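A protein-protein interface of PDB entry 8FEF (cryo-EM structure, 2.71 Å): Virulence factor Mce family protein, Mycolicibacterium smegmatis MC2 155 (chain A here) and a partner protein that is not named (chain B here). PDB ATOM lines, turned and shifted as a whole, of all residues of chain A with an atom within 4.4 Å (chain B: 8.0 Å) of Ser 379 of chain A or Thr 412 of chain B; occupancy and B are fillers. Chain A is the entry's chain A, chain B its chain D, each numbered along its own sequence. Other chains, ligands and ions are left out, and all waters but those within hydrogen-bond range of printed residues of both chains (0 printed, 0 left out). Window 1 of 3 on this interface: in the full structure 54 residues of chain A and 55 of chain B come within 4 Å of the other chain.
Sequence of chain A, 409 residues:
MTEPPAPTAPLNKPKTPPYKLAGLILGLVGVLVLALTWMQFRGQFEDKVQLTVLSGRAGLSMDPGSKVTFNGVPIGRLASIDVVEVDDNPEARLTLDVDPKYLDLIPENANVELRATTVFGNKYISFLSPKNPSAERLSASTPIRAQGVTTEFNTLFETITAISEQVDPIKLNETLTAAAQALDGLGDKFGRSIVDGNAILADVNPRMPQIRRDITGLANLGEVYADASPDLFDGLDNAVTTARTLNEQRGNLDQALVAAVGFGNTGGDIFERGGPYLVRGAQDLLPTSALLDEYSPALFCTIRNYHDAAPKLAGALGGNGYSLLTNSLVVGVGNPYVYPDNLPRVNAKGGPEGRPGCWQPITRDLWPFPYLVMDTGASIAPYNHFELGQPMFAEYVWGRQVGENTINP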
ATOM      1  N   ASN A 342     -13.054 -12.084  36.528  1.00  0.00           N
ATOM      2  CA  ASN A 342     -14.201 -12.729  35.908  1.00  0.00           C
ATOM      3  C   ASN A 342     -15.517 -12.558  36.633  1.00  0.00           C
ATOM      4  O   ASN A 342     -16.508 -13.142  36.229  1.00  0.00           O
ATOM      5  CB  ASN A 342     -13.936 -14.208  35.654  1.00  0.00           C
ATOM      6  CG  ASN A 342     -13.034 -14.439  34.469  1.00  0.00           C
ATOM      7  OD1 ASN A 342     -12.188 -15.316  34.500  1.00  0.00           O
ATOM      8  ND2 ASN A 342     -13.207 -13.654  33.426  1.00  0.00           N
ATOM      9  N   TYR A 371     -19.855 -15.246  17.448  1.00  0.00           N
ATOM     10  CA  TYR A 371     -19.838 -14.973  18.878  1.00  0.00           C
ATOM     11  C   TYR A 371     -19.886 -13.471  19.124  1.00  0.00           C
ATOM     12  O   TYR A 371     -19.131 -12.706  18.519  1.00  0.00           O
ATOM     13  CB  TYR A 371     -18.592 -15.579  19.517  1.00  0.00           C
ATOM     14  CG  TYR A 371     -18.566 -15.434  21.016  1.00  0.00           C
ATOM     15  CD1 TYR A 371     -19.320 -16.269  21.820  1.00  0.00           C
ATOM     16  CD2 TYR A 371     -17.801 -14.455  21.625  1.00  0.00           C
ATOM     17  CE1 TYR A 371     -19.309 -16.139  23.187  1.00  0.00           C
ATOM     18  CE2 TYR A 371     -17.784 -14.315  22.994  1.00  0.00           C
ATOM     19  CZ  TYR A 371     -18.538 -15.161  23.770  1.00  0.00           C
ATOM     20  OH  TYR A 371     -18.528 -15.031  25.138  1.00  0.00           O
ATOM     21  N   VAL A 373     -19.443 -10.329  21.641  1.00  0.00           N
ATOM     22  CA  VAL A 373     -18.670  -9.930  22.811  1.00  0.00           C
ATOM     23  C   VAL A 373     -19.306  -8.681  23.402  1.00  0.00           C
ATOM     24  O   VAL A 373     -19.489  -7.677  22.703  1.00  0.00           O
ATOM     25  CB  VAL A 373     -17.198  -9.685  22.446  1.00  0.00           C
ATOM     26  CG1 VAL A 373     -16.425  -9.196  23.654  1.00  0.00           C
ATOM     27  CG2 VAL A 373     -16.576 -10.953  21.891  1.00  0.00           C
ATOM     28  N   GLY A 377     -17.886  -9.347  31.979  1.00  0.00           N
ATOM     29  CA  GLY A 377     -16.886  -9.848  32.884  1.00  0.00           C
ATOM     30  C   GLY A 377     -16.383 -11.224  32.523  1.00  0.00           C
ATOM     31  O   GLY A 377     -15.551 -11.769  33.251  1.00  0.00           O
ATOM     32  N   ALA A 378     -16.844 -11.796  31.414  1.00  0.00           N
ATOM     33  CA  ALA A 378     -16.397 -13.107  30.974  1.00  0.00           C
ATOM     34  C   ALA A 378     -16.573 -13.208  29.469  1.00  0.00           C
ATOM     35  O   ALA A 378     -17.505 -12.637  28.898  1.00  0.00           O
ATOM     36  CB  ALA A 378     -17.164 -14.231  31.672  1.00  0.00           C
ATOM     37  N   SER A 379     -15.665 -13.943  28.831  1.00  0.00           N
ATOM     38  CA  SER A 379     -15.687 -14.110  27.387  1.00  0.00           C
ATOM     39  C   SER A 379     -15.001 -15.421  27.036  1.00  0.00           C
ATOM     40  O   SER A 379     -14.277 -16.000  27.850  1.00  0.00           O
ATOM     41  CB  SER A 379     -15.008 -12.932  26.679  1.00  0.00           C
ATOM     42  OG  SER A 379     -14.948 -13.136  25.281  1.00  0.00           O
ATOM     43  N   ILE A 380     -15.253 -15.898  25.817  1.00  0.00           N
ATOM     44  CA  ILE A 380     -14.563 -17.077  25.305  1.00  0.00           C
ATOM     45  C   ILE A 380     -13.951 -16.721  23.960  1.00  0.00           C
ATOM     46  O   ILE A 380     -13.586 -17.602  23.175  1.00  0.00           O
ATOM     47  CB  ILE A 380     -15.496 -18.297  25.183  1.00  0.00           C
ATOM     48  CG1 ILE A 380     -16.588 -18.042  24.146  1.00  0.00           C
ATOM     49  CG2 ILE A 380     -16.087 -18.669  26.533  1.00  0.00           C
ATOM     50  CD1 ILE A 380     -17.468 -19.238  23.885  1.00  0.00           C
ATOM     51  N   ALA A 381     -13.837 -15.420  23.691  1.00  0.00           N
ATOM     52  CA  ALA A 381     -13.190 -14.963  22.465  1.00  0.00           C
ATOM     53  C   ALA A 381     -11.738 -15.410  22.296  1.00  0.00           C
ATOM     54  O   ALA A 381     -11.380 -15.795  21.170  1.00  0.00           O
ATOM     55  CB  ALA A 381     -13.291 -13.436  22.370  1.00  0.00           C
ATOM     56  N   PRO A 382     -10.860 -15.382  23.305  1.00  0.00           N
ATOM     57  CA  PRO A 382      -9.449 -15.702  23.054  1.00  0.00           C
ATOM     58  C   PRO A 382      -9.143 -17.179  22.859  1.00  0.00           C
ATOM     59  O   PRO A 382      -7.964 -17.541  22.834  1.00  0.00           O
ATOM     60  CB  PRO A 382      -8.759 -15.178  24.321  1.00  0.00           C
ATOM     61  CG  PRO A 382      -9.759 -15.368  25.363  1.00  0.00           C
ATOM     62  CD  PRO A 382     -11.052 -14.994  24.717  1.00  0.00           C
ATOM     63  N   ILE A 407      -6.198 -14.375  32.435  1.00  0.00           N
ATOM     64  CA  ILE A 407      -7.298 -13.991  31.567  1.00  0.00           C
ATOM     65  C   ILE A 407      -6.861 -13.939  30.113  1.00  0.00           C
ATOM     66  O   ILE A 407      -7.647 -13.546  29.245  1.00  0.00           O
ATOM     67  CB  ILE A 407      -7.908 -12.648  31.997  1.00  0.00           C
ATOM     68  CG1 ILE A 407      -6.970 -11.498  31.625  1.00  0.00           C
ATOM     69  CG2 ILE A 407      -8.186 -12.649  33.484  1.00  0.00           C
ATOM     70  CD1 ILE A 407      -7.573 -10.138  31.825  1.00  0.00           C
ATOM     71  N   PRO A 409      -5.425 -16.535  27.689  1.00  0.00           N
ATOM     72  CA  PRO A 409      -4.967 -17.852  27.249  1.00  0.00           C
ATOM     73  C   PRO A 409      -4.331 -17.783  25.871  1.00  0.00           C
ATOM     74  O   PRO A 409      -4.608 -16.874  25.092  1.00  0.00           O
ATOM     75  CB  PRO A 409      -6.254 -18.675  27.220  1.00  0.00           C
ATOM     76  CG  PRO A 409      -7.315 -17.681  26.942  1.00  0.00           C
ATOM     77  CD  PRO A 409      -6.892 -16.412  27.622  1.00  0.00           C
ATOM     78  OXT PRO A 409      -3.523 -18.631  25.507  1.00  0.00           O
ATOM     79  N   ALA B 311     -25.992 -14.375  30.303  1.00  0.00           N
ATOM     80  CA  ALA B 311     -24.588 -14.213  29.956  1.00  0.00           C
ATOM     81  C   ALA B 311     -23.822 -15.527  30.085  1.00  0.00           C
ATOM     82  O   ALA B 311     -23.046 -15.900  29.194  1.00  0.00           O
ATOM     83  CB  ALA B 311     -23.987 -13.144  30.853  1.00  0.00           C
ATOM     84  N   LEU B 314     -24.734 -17.884  27.389  1.00  0.00           N
ATOM     85  CA  LEU B 314     -24.128 -17.467  26.134  1.00  0.00           C
ATOM     86  C   LEU B 314     -22.627 -17.711  26.110  1.00  0.00           C
ATOM     87  O   LEU B 314     -22.030 -17.702  25.029  1.00  0.00           O
ATOM     88  CB  LEU B 314     -24.414 -15.989  25.858  1.00  0.00           C
ATOM     89  CG  LEU B 314     -25.804 -15.639  25.322  1.00  0.00           C
ATOM     90  CD1 LEU B 314     -25.820 -14.226  24.782  1.00  0.00           C
ATOM     91  CD2 LEU B 314     -26.234 -16.621  24.247  1.00  0.00           C
ATOM     92  N   ASN B 315     -22.004 -17.928  27.267  1.00  0.00           N
ATOM     93  CA  ASN B 315     -20.581 -18.247  27.316  1.00  0.00           C
ATOM     94  C   ASN B 315     -20.285 -19.742  27.302  1.00  0.00           C
ATOM     95  O   ASN B 315     -19.109 -20.118  27.322  1.00  0.00           O
ATOM     96  CB  ASN B 315     -19.933 -17.615  28.550  1.00  0.00           C
ATOM     97  CG  ASN B 315     -19.548 -16.170  28.327  1.00  0.00           C
ATOM     98  OD1 ASN B 315     -19.134 -15.789  27.233  1.00  0.00           O
ATOM     99  ND2 ASN B 315     -19.681 -15.355  29.365  1.00  0.00           N
ATOM    100  N   MET B 389     -12.451 -22.935  20.846  1.00  0.00           N
ATOM    101  CA  MET B 389     -13.893 -22.724  20.822  1.00  0.00           C
ATOM    102  C   MET B 389     -14.309 -21.810  19.676  1.00  0.00           C
ATOM    103  O   MET B 389     -15.317 -22.068  19.011  1.00  0.00           O
ATOM    104  CB  MET B 389     -14.370 -22.151  22.156  1.00  0.00           C
ATOM    105  CG  MET B 389     -14.193 -23.086  23.337  1.00  0.00           C
ATOM    106  SD  MET B 389     -15.028 -22.478  24.813  1.00  0.00           S
ATOM    107  CE  MET B 389     -14.544 -23.715  26.012  1.00  0.00           C
ATOM    108  N   THR B 390     -13.556 -20.744  19.428  1.00  0.00           N
ATOM    109  CA  THR B 390     -13.871 -19.779  18.382  1.00  0.00           C
ATOM    110  C   THR B 390     -12.684 -19.630  17.434  1.00  0.00           C
ATOM    111  O   THR B 390     -11.627 -20.234  17.620  1.00  0.00           O
ATOM    112  CB  THR B 390     -14.247 -18.417  18.975  1.00  0.00           C
ATOM    113  OG1 THR B 390     -13.059 -17.711  19.349  1.00  0.00           O
ATOM    114  CG2 THR B 390     -15.131 -18.576  20.199  1.00  0.00           C
ATOM    115  N   ILE B 395     -15.480 -13.698  15.492  1.00  0.00           N
ATOM    116  CA  ILE B 395     -15.781 -12.842  16.632  1.00  0.00           C
ATOM    117  C   ILE B 395     -16.461 -11.567  16.157  1.00  0.00           C
ATOM    118  O   ILE B 395     -15.984 -10.890  15.237  1.00  0.00           O
ATOM    119  CB  ILE B 395     -14.504 -12.528  17.422  1.00  0.00           C
ATOM    120  CG1 ILE B 395     -13.778 -13.817  17.793  1.00  0.00           C
ATOM    121  CG2 ILE B 395     -14.839 -11.756  18.678  1.00  0.00           C
ATOM    122  CD1 ILE B 395     -14.610 -14.758  18.628  1.00  0.00           C
ATOM    123  N   ALA B 396     -17.587 -11.239  16.784  1.00  0.00           N
ATOM    124  CA  ALA B 396     -18.282  -9.981  16.575  1.00  0.00           C
ATOM    125  C   ALA B 396     -18.462  -9.298  17.921  1.00  0.00           C
ATOM    126  O   ALA B 396     -18.569  -9.958  18.958  1.00  0.00           O
ATOM    127  CB  ALA B 396     -19.640 -10.191  15.903  1.00  0.00           C
ATOM    128  N   TYR B 397     -18.478  -7.969  17.907  1.00  0.00           N
ATOM    129  CA  TYR B 397     -18.504  -7.181  19.130  1.00  0.00           C
ATOM    130  C   TYR B 397     -19.831  -6.451  19.250  1.00  0.00           C
ATOM    131  O   TYR B 397     -20.305  -5.852  18.279  1.00  0.00           O
ATOM    132  CB  TYR B 397     -17.337  -6.194  19.160  1.00  0.00           C
ATOM    133  CG  TYR B 397     -15.993  -6.880  19.119  1.00  0.00           C
ATOM    134  CD1 TYR B 397     -15.465  -7.479  20.250  1.00  0.00           C
ATOM    135  CD2 TYR B 397     -15.261  -6.942  17.943  1.00  0.00           C
ATOM    136  CE1 TYR B 397     -14.244  -8.116  20.216  1.00  0.00           C
ATOM    137  CE2 TYR B 397     -14.038  -7.575  17.899  1.00  0.00           C
ATOM    138  CZ  TYR B 397     -13.535  -8.160  19.037  1.00  0.00           C
ATOM    139  OH  TYR B 397     -12.316  -8.792  18.997  1.00  0.00           O
ATOM    140  N   LYS B 409      -5.249  -7.925  21.155  1.00  0.00           N
ATOM    141  CA  LYS B 409      -6.183  -9.034  21.026  1.00  0.00           C
ATOM    142  C   LYS B 409      -7.075  -9.125  22.257  1.00  0.00           C
ATOM    143  O   LYS B 409      -6.732  -8.645  23.339  1.00  0.00           O
ATOM    144  CB  LYS B 409      -5.453 -10.364  20.812  1.00  0.00           C
ATOM    145  CG  LYS B 409      -4.703 -10.875  22.025  1.00  0.00           C
ATOM    146  CD  LYS B 409      -3.930 -12.134  21.684  1.00  0.00           C
ATOM    147  CE  LYS B 409      -3.301 -12.748  22.914  1.00  0.00           C
ATOM    148  NZ  LYS B 409      -2.548 -13.984  22.580  1.00  0.00           N
ATOM    149  N   ASP B 410      -8.231  -9.755  22.075  1.00  0.00           N
ATOM    150  CA  ASP B 410      -9.232  -9.852  23.129  1.00  0.00           C
ATOM    151  C   ASP B 410      -8.851 -10.920  24.149  1.00  0.00           C
ATOM    152  O   ASP B 410      -8.136 -11.878  23.844  1.00  0.00           O
ATOM    153  CB  ASP B 410     -10.607 -10.159  22.533  1.00  0.00           C
ATOM    154  CG  ASP B 410     -11.743  -9.848  23.490  1.00  0.00           C
ATOM    155  OD1 ASP B 410     -12.045  -8.654  23.689  1.00  0.00           O
ATOM    156  OD2 ASP B 410     -12.334 -10.794  24.045  1.00  0.00           O
ATOM    157  N   THR B 411      -9.342 -10.744  25.371  1.00  0.00           N
ATOM    158  CA  THR B 411      -9.068 -11.627  26.497  1.00  0.00           C
ATOM    159  C   THR B 411     -10.379 -12.190  27.036  1.00  0.00           C
ATOM    160  O   THR B 411     -11.465 -11.861  26.555  1.00  0.00           O
ATOM    161  CB  THR B 411      -8.317 -10.878  27.596  1.00  0.00           C
ATOM    162  OG1 THR B 411      -9.103  -9.763  28.033  1.00  0.00           O
ATOM    163  CG2 THR B 411      -7.004 -10.371  27.072  1.00  0.00           C
ATOM    164  N   THR B 412     -10.273 -13.051  28.054  1.00  0.00           N
ATOM    165  CA  THR B 412     -11.474 -13.630  28.643  1.00  0.00           C
ATOM    166  C   THR B 412     -12.322 -12.588  29.356  1.00  0.00           C
ATOM    167  O   THR B 412     -13.492 -12.854  29.642  1.00  0.00           O
ATOM    168  CB  THR B 412     -11.126 -14.755  29.620  1.00  0.00           C
ATOM    169  OG1 THR B 412     -10.508 -14.208  30.788  1.00  0.00           O
ATOM    170  CG2 THR B 412     -10.191 -15.755  28.977  1.00  0.00           C
ATOM    171  N   VAL B 413     -11.762 -11.420  29.653  1.00  0.00           N
ATOM    172  CA  VAL B 413     -12.510 -10.302  30.218  1.00  0.00           C
ATOM    173  C   VAL B 413     -12.712  -9.283  29.100  1.00  0.00           C
ATOM    174  O   VAL B 413     -11.724  -8.691  28.636  1.00  0.00           O
ATOM    175  CB  VAL B 413     -11.781  -9.676  31.413  1.00  0.00           C
ATOM    176  CG1 VAL B 413     -12.623  -8.576  32.030  1.00  0.00           C
ATOM    177  CG2 VAL B 413     -11.453 -10.735  32.444  1.00  0.00           C
ATOM    178  N   PRO B 414     -13.937  -9.078  28.616  1.00  0.00           N
ATOM    179  CA  PRO B 414     -14.149  -8.119  27.526  1.00  0.00           C
ATOM    180  C   PRO B 414     -13.721  -6.718  27.931  1.00  0.00           C
ATOM    181  O   PRO B 414     -13.923  -6.291  29.067  1.00  0.00           O
ATOM    182  CB  PRO B 414     -15.659  -8.195  27.277  1.00  0.00           C
ATOM    183  CG  PRO B 414     -16.077  -9.508  27.838  1.00  0.00           C
ATOM    184  CD  PRO B 414     -15.186  -9.749  29.012  1.00  0.00           C
ATOM    185  N   GLY B 415     -13.120  -6.003  26.985  1.00  0.00           N
ATOM    186  CA  GLY B 415     -12.645  -4.662  27.218  1.00  0.00           C
ATOM    187  C   GLY B 415     -11.194  -4.559  27.639  1.00  0.00           C
ATOM    188  O   GLY B 415     -10.629  -3.463  27.586  1.00  0.00           O
ATOM    189  N   ILE B 416     -10.575  -5.660  28.052  1.00  0.00           N
ATOM    190  CA  ILE B 416      -9.155  -5.697  28.380  1.00  0.00           C
ATOM    191  C   ILE B 416      -8.423  -6.314  27.196  1.00  0.00           C
ATOM    192  O   ILE B 416      -8.682  -7.467  26.830  1.00  0.00           O
ATOM    193  CB  ILE B 416      -8.893  -6.487  29.670  1.00  0.00           C
ATOM    194  CG1 ILE B 416      -9.582  -5.814  30.857  1.00  0.00           C
ATOM    195  CG2 ILE B 416      -7.402  -6.620  29.926  1.00  0.00           C
ATOM    196  CD1 ILE B 416      -9.278  -6.465  32.181  1.00  0.00           C
ATOM    197  N   SER B 418      -4.971  -7.474  25.320  1.00  0.00           N
ATOM    198  CA  SER B 418      -3.581  -7.884  25.467  1.00  0.00           C
ATOM    199  C   SER B 418      -2.775  -7.437  24.254  1.00  0.00           C
ATOM    200  O   SER B 418      -3.233  -6.653  23.423  1.00  0.00           O
ATOM    201  CB  SER B 418      -3.481  -9.393  25.660  1.00  0.00           C
ATOM    202  OG  SER B 418      -3.935  -9.776  26.938  1.00  0.00           O
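CE1 of Tyr 371 of chain A touches O of Leu 314 of chain B, at 3.6 Å.
Ala 378 of chain A touches Asn 315 of chain B.
Ala 378 of chain A touches Pro 414 of chain B.
Ser 379 of chain A touches Asp 410 of chain B.
Ser 379 of chain A touches Pro 414 of chain B.
Ile 380 of chain A touches Asn 315 of chain B.
Ala 381 of chain A touches Asp 410 of chain B (CB to OD2, 3.3 Å).
Pro 382 of chain A touches Asp 410 of chain B (CB to O, 3.4 Å).
Pro 382 of chain A touches Thr 411 of chain B (CG to C, 3.6 Å).
CG2 of Thr 412 of chain B touches CD of Pro 409 of chain A, 3.6 Å away.
Of chain B, only Asn 315, Thr 412 and Pro 414 come within 4 Å of Ala 378 of chain A.
Ser 379 of chain A touches just these residues of chain B: Asn 315 (3.8 Å), Asp 410 (3.7 Å), Thr 411 (3.7 Å), Thr 412 (2.6 Å) and Pro 414 (3.8 Å).
Of the printed residues of chain B, Pro 382 of chain A touches Asp 410, Thr 411 and Thr 412.
Of chain A, only Asn 342, Ala 378, Ser 379, Pro 382, Ile 407 and Pro 409 come within 4 Å of Thr 412 of chain B.
Of the printed residues of chain A, Pro 414 of chain B touches Val 373, Gly 377, Ala 378 and Ser 379.
The nearest residue of chain A that does not touch Thr 412 of chain B is Gly 377 of chain A (4.3 Å).
The backbone carbonyl oxygen of Gly 377 of chain A sits at hydrogen-bond distance from the side-chain amide nitrogen of Asn 342 of chain A.
N of Ile 380 of chain A lies within hydrogen-bond range of OH of Tyr 371 of chain A.
The backbone NH of Ala 381 of chain A is in hydrogen-bond range of the side-chain hydroxyl of Ser 379 of chain A.
The side-chain amide nitrogen (ND2) of Asn 315 of chain B sits at hydrogen-bond distance from the backbone carbonyl oxygen (O) of Ala 311 of chain B, 3.4 Å away.
The side-chain hydroxyl of Thr 411 of chain B is in hydrogen-bond range of the backbone carbonyl oxygen of Val 413 of chain B.
The side-chain hydroxyl (OG1) of Thr 411 of chain B lies within hydrogen-bond range of the backbone carbonyl oxygen (O) of Ile 416 of chain B (2.6 Å).
Printed residues of chain A that touch a printed residue of chain B: Asn 342, Tyr 371, Val 373, Gly 377, Ala 378, Ser 379, Ile 380, Ala 381, Pro 382, Ile 407 and Pro 409.
Hydrophobic or aromatic side chains of chain A within 4 Å of the printed part of chain B: Tyr 371, Val 373, Ala 378, Ile 380, Ala 381, Pro 382, Ile 407 and Pro 409.
Along chain A the printed residues that touch a printed residue of chain B span positions 342 to 409.
Hydrophobic or aromatic side chains of chain B within 4 Å of the printed part of chain A: Ile 395, Ala 396, Tyr 397, Val 413 and Pro 414.
Along chain B the printed residues that touch a printed residue of chain A span positions 314 to 414.
Among the printed residues, 30 pairs touch across the chains.
Among the printed residues, no Asp or Glu carboxylate lies within 4 Å of a Lys or Arg side-chain nitrogen of the other chain.
The backbone carbonyl oxygen of Tyr 371 of chain A lies within hydrogen-bond range of the backbone NH of Ala 396 of chain B (2.7 Å).
The backbone carbonyl oxygen of Ala 396 of chain B sits at hydrogen-bond distance from the backbone NH of Val 373 of chain A.
The backbone carbonyl oxygen of Thr 412 of chain B is in hydrogen-bond range of the backbone NH of Ser 379 of chain A (2.6 Å).
OG1 of Thr 390 of chain B lies within hydrogen-bond range of O of Ala 381 of chain A (3.1 Å).
The backbone carbonyl oxygen (O) of Ile 407 of chain A is in hydrogen-bond range of the backbone NH (N) of Thr 412 of chain B (2.9 Å).
OH of Tyr 371 of chain A sits close to OD1 of Asn 315 of chain B (2.3 Å).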
